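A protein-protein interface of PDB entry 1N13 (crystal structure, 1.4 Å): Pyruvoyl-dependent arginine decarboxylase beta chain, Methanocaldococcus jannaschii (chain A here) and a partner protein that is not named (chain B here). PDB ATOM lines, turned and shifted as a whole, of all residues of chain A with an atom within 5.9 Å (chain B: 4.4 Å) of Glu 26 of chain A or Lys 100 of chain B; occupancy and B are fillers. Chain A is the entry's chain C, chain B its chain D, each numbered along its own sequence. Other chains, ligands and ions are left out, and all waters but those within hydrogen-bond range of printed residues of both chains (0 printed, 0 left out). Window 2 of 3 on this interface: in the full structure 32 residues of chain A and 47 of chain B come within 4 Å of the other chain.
The side-chain hydroxyl (OG) of Ser 24 of chain A sits at hydrogen-bond distance from a ring nitrogen (ND1) of His 96 of chain B (3.1 Å). OE1 of Glu 26 of chain A is in hydrogen-bond range of NE2 of His 96 of chain B, 2.8 Å away. The side-chain carboxylate (OE1) of Glu 26 of chain A lies within hydrogen-bond range of the backbone NH (N) of Glu 99 of chain B (2.9 Å). The side-chain carboxylate (OE2) of Glu 26 of chain A is in hydrogen-bond range of the backbone NH (N) of Lys 100 of chain B (3.0 Å). The side-chain carboxylate of Glu 26 of chain A lies within hydrogen-bond range of the backbone NH of Leu 101 of chain B. N of Gly 27 of chain A lies within hydrogen-bond range of O of Leu 101 of chain B.
The backbone NH (N) of Ser 30 of chain B lies within hydrogen-bond range of the backbone carbonyl oxygen (O) of Gly 102 of chain B (2.9 Å).
Among the printed residues, merely in contact across the chains: Ser 25 of chain A with Gly 102 of chain B (3.3 Å), Glu 26 of chain A with Val 98 of chain B (3.6 Å), Ala 33 of chain A with Leu 101 of chain B (3.8 Å), Glu 26 of chain A with Gly 102 of chain B (3.8 Å), Ser 25 of chain A with His 96 of chain B (3.8 Å) and Glu 26 of chain A with Thr 97 of chain B (3.96 Å).
Of the printed residues of chain B, Ser 25 of chain A touches His 96 and Gly 102. Printed residues of chain A within 4 Å of Thr 97 of chain B: Glu 26 (3.96 Å). Lys 100 of chain B touches just one residue of chain A: Glu 26. Printed residues of chain A within 4 Å of Leu 101 of chain B: Glu 26 (3.0 Å), Gly 27 (2.9 Å) and Ala 33 (3.8 Å). The nearest residue of chain A that does not touch Lys 100 of chain B is Gly 27 of chain A (5.7 Å). The nearest printed residue of chain A that does not touch His 96 of chain B is Gly 27 of chain A (6.7 Å).
Of the 8 printed residues of chain A, 5 touch a printed residue of chain B. Hydrophobic or aromatic side chains of chain A that line the printed part of chain B: Ala 33. Printed residues of chain B that touch a printed residue of chain A: His 96, Thr 97, Val 98, Glu 99, Lys 100, Leu 101 and Gly 102. Hydrophobic or aromatic side chains of chain B that line the printed part of chain A: His 96 and Leu 101. Among the printed residues, no Asp or Glu carboxylate lies within 4 Å of a Lys or Arg side-chain nitrogen of the other chain.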
ATOM      1  N   SER A  24       3.742 -26.181  23.948  1.00  0.00           N
ATOM      2  CA  SER A  24       2.390 -26.013  23.446  1.00  0.00           C
ATOM      3  C   SER A  24       2.008 -24.555  23.587  1.00  0.00           C
ATOM      4  O   SER A  24       2.630 -23.809  24.352  1.00  0.00           O
ATOM      5  CB  SER A  24       1.404 -26.900  24.212  1.00  0.00           C
ATOM      6  OG  SER A  24       1.210 -26.433  25.535  1.00  0.00           O
ATOM      7  N   SER A  25       0.993 -24.148  22.836  1.00  0.00           N
ATOM      8  CA  SER A  25       0.540 -22.770  22.879  1.00  0.00           C
ATOM      9  C   SER A  25      -0.778 -22.589  22.164  1.00  0.00           C
ATOM     10  O   SER A  25      -1.165 -23.396  21.317  1.00  0.00           O
ATOM     11  CB  SER A  25       1.581 -21.855  22.222  1.00  0.00           C
ATOM     12  OG  SER A  25       1.168 -20.493  22.196  1.00  0.00           O
ATOM     13  N   GLU A  26      -1.483 -21.532  22.552  1.00  0.00           N
ATOM     14  CA  GLU A  26      -2.732 -21.168  21.909  1.00  0.00           C
ATOM     15  C   GLU A  26      -2.280 -20.223  20.796  1.00  0.00           C
ATOM     16  O   GLU A  26      -1.118 -19.806  20.765  1.00  0.00           O
ATOM     17  CB  GLU A  26      -3.654 -20.432  22.885  1.00  0.00           C
ATOM     18  CG  GLU A  26      -4.368 -21.329  23.891  1.00  0.00           C
ATOM     19  CD  GLU A  26      -5.549 -22.079  23.292  1.00  0.00           C
ATOM     20  OE1 GLU A  26      -5.615 -23.314  23.449  1.00  0.00           O
ATOM     21  OE2 GLU A  26      -6.422 -21.434  22.674  1.00  0.00           O
ATOM     22  N   GLY A  27      -3.181 -19.896  19.881  1.00  0.00           N
ATOM     23  CA  GLY A  27      -2.823 -19.000  18.796  1.00  0.00           C
ATOM     24  C   GLY A  27      -4.042 -18.546  18.028  1.00  0.00           C
ATOM     25  O   GLY A  27      -5.033 -19.267  17.952  1.00  0.00           O
ATOM     26  N   GLU A  28      -3.962 -17.355  17.446  1.00  0.00           N
ATOM     27  CA  GLU A  28      -5.073 -16.804  16.678  1.00  0.00           C
ATOM     28  C   GLU A  28      -5.282 -17.532  15.352  1.00  0.00           C
ATOM     29  O   GLU A  28      -6.364 -17.481  14.770  1.00  0.00           O
ATOM     30  CB  GLU A  28      -4.874 -15.304  16.469  1.00  0.00           C
ATOM     31  CG  GLU A  28      -5.004 -14.514  17.768  1.00  0.00           C
ATOM     32  CD  GLU A  28      -4.656 -13.048  17.619  1.00  0.00           C
ATOM     33  OE1 GLU A  28      -3.731 -12.587  18.323  1.00  0.00           O
ATOM     34  OE2 GLU A  28      -5.306 -12.354  16.808  1.00  0.00           O
ATOM     35  N   ASN A  32       0.230 -19.392  13.928  1.00  0.00           N
ATOM     36  CA  ASN A  32       0.611 -18.615  15.105  1.00  0.00           C
ATOM     37  C   ASN A  32       0.669 -19.508  16.341  1.00  0.00           C
ATOM     38  O   ASN A  32       1.496 -19.290  17.226  1.00  0.00           O
ATOM     39  CB  ASN A  32      -0.350 -17.445  15.339  1.00  0.00           C
ATOM     40  CG  ASN A  32      -0.124 -16.305  14.360  1.00  0.00           C
ATOM     41  OD1 ASN A  32      -1.036 -15.896  13.645  1.00  0.00           O
ATOM     42  ND2 ASN A  32       1.101 -15.784  14.327  1.00  0.00           N
ATOM     43  N   ALA A  33      -0.204 -20.512  16.390  1.00  0.00           N
ATOM     44  CA  ALA A  33      -0.225 -21.461  17.508  1.00  0.00           C
ATOM     45  C   ALA A  33       1.016 -22.346  17.421  1.00  0.00           C
ATOM     46  O   ALA A  33       1.643 -22.654  18.434  1.00  0.00           O
ATOM     47  CB  ALA A  33      -1.489 -22.315  17.461  1.00  0.00           C
ATOM     48  N   GLY A  36       3.906 -20.344  18.473  1.00  0.00           N
ATOM     49  CA  GLY A  36       3.887 -20.238  19.921  1.00  0.00           C
ATOM     50  C   GLY A  36       4.396 -21.497  20.602  1.00  0.00           C
ATOM     51  O   GLY A  36       5.062 -21.423  21.632  1.00  0.00           O
ATOM     52  N   SER B  30      -5.557 -28.047  17.121  1.00  0.00           N
ATOM     53  CA  SER B  30      -6.989 -28.270  17.291  1.00  0.00           C
ATOM     54  C   SER B  30      -7.738 -27.006  17.678  1.00  0.00           C
ATOM     55  O   SER B  30      -7.248 -26.202  18.468  1.00  0.00           O
ATOM     56  CB  SER B  30      -7.238 -29.347  18.346  1.00  0.00           C
ATOM     57  OG  SER B  30      -8.619 -29.439  18.657  1.00  0.00           O
ATOM     58  N   ASP B  31      -8.936 -26.848  17.117  1.00  0.00           N
ATOM     59  CA  ASP B  31      -9.784 -25.697  17.407  1.00  0.00           C
ATOM     60  C   ASP B  31     -11.050 -26.121  18.150  1.00  0.00           C
ATOM     61  O   ASP B  31     -12.070 -25.433  18.103  1.00  0.00           O
ATOM     62  CB  ASP B  31     -10.134 -24.931  16.119  1.00  0.00           C
ATOM     63  CG  ASP B  31     -10.916 -25.771  15.105  1.00  0.00           C
ATOM     64  OD1 ASP B  31     -11.114 -26.987  15.314  1.00  0.00           O
ATOM     65  OD2 ASP B  31     -11.336 -25.197  14.080  1.00  0.00           O
ATOM     66  N   HIS B  96      -1.791 -30.388  25.720  1.00  0.00           N
ATOM     67  CA  HIS B  96      -2.390 -29.065  25.733  1.00  0.00           C
ATOM     68  C   HIS B  96      -3.901 -29.191  25.668  1.00  0.00           C
ATOM     69  O   HIS B  96      -4.433 -29.976  24.883  1.00  0.00           O
ATOM     70  CB  HIS B  96      -1.885 -28.250  24.536  1.00  0.00           C
ATOM     71  CG  HIS B  96      -2.417 -26.851  24.484  1.00  0.00           C
ATOM     72  ND1 HIS B  96      -1.779 -25.790  25.088  1.00  0.00           N
ATOM     73  CD2 HIS B  96      -3.522 -26.338  23.892  1.00  0.00           C
ATOM     74  CE1 HIS B  96      -2.468 -24.682  24.872  1.00  0.00           C
ATOM     75  NE2 HIS B  96      -3.530 -24.988  24.149  1.00  0.00           N
ATOM     76  N   THR B  97      -4.585 -28.462  26.542  1.00  0.00           N
ATOM     77  CA  THR B  97      -6.040 -28.465  26.548  1.00  0.00           C
ATOM     78  C   THR B  97      -6.456 -27.213  25.790  1.00  0.00           C
ATOM     79  O   THR B  97      -6.170 -26.093  26.216  1.00  0.00           O
ATOM     80  CB  THR B  97      -6.615 -28.444  27.978  1.00  0.00           C
ATOM     81  OG1 THR B  97      -6.166 -29.607  28.685  1.00  0.00           O
ATOM     82  CG2 THR B  97      -8.140 -28.455  27.934  1.00  0.00           C
ATOM     83  N   VAL B  98      -7.080 -27.417  24.636  1.00  0.00           N
ATOM     84  CA  VAL B  98      -7.514 -26.317  23.785  1.00  0.00           C
ATOM     85  C   VAL B  98      -8.553 -25.400  24.419  1.00  0.00           C
ATOM     86  O   VAL B  98      -9.547 -25.861  24.985  1.00  0.00           O
ATOM     87  CB  VAL B  98      -8.067 -26.836  22.444  1.00  0.00           C
ATOM     88  CG1 VAL B  98      -8.539 -25.670  21.575  1.00  0.00           C
ATOM     89  CG2 VAL B  98      -7.003 -27.643  21.718  1.00  0.00           C
ATOM     90  N   GLU B  99      -8.289 -24.099  24.348  1.00  0.00           N
ATOM     91  CA  GLU B  99      -9.209 -23.096  24.865  1.00  0.00           C
ATOM     92  C   GLU B  99     -10.002 -22.601  23.659  1.00  0.00           C
ATOM     93  O   GLU B  99     -11.233 -22.619  23.663  1.00  0.00           O
ATOM     94  CB  GLU B  99      -8.448 -21.945  25.520  1.00  0.00           C
ATOM     95  CG  GLU B  99      -7.611 -22.367  26.717  1.00  0.00           C
ATOM     96  CD  GLU B  99      -6.997 -21.188  27.445  1.00  0.00           C
ATOM     97  OE1 GLU B  99      -7.724 -20.519  28.210  1.00  0.00           O
ATOM     98  OE2 GLU B  99      -5.789 -20.933  27.255  1.00  0.00           O
ATOM     99  N   LYS B 100      -9.282 -22.211  22.609  1.00  0.00           N
ATOM    100  CA  LYS B 100      -9.897 -21.736  21.373  1.00  0.00           C
ATOM    101  C   LYS B 100      -9.209 -22.396  20.179  1.00  0.00           C
ATOM    102  O   LYS B 100      -9.863 -22.964  19.305  1.00  0.00           O
ATOM    103  CB  LYS B 100      -9.784 -20.214  21.265  1.00  0.00           C
ATOM    104  CG  LYS B 100     -10.711 -19.605  20.226  1.00  0.00           C
ATOM    105  CD  LYS B 100     -10.633 -18.084  20.235  1.00  0.00           C
ATOM    106  CE  LYS B 100     -11.755 -17.461  19.414  1.00  0.00           C
ATOM    107  NZ  LYS B 100     -11.729 -17.889  17.990  1.00  0.00           N
ATOM    108  N   LEU B 101      -7.882 -22.319  20.157  1.00  0.00           N
ATOM    109  CA  LEU B 101      -7.082 -22.911  19.089  1.00  0.00           C
ATOM    110  C   LEU B 101      -5.681 -23.154  19.643  1.00  0.00           C
ATOM    111  O   LEU B 101      -4.949 -22.208  19.935  1.00  0.00           O
ATOM    112  CB  LEU B 101      -7.033 -21.968  17.878  1.00  0.00           C
ATOM    113  CG  LEU B 101      -6.606 -22.520  16.512  1.00  0.00           C
ATOM    114  CD1 LEU B 101      -6.998 -21.530  15.428  1.00  0.00           C
ATOM    115  CD2 LEU B 101      -5.113 -22.802  16.462  1.00  0.00           C
ATOM    116  N   GLY B 102      -5.320 -24.426  19.793  1.00  0.00           N
ATOM    117  CA  GLY B 102      -4.014 -24.766  20.332  1.00  0.00           C
ATOM    118  C   GLY B 102      -3.175 -25.750  19.541  1.00  0.00           C
ATOM    119  O   GLY B 102      -3.668 -26.462  18.668  1.00  0.00           O
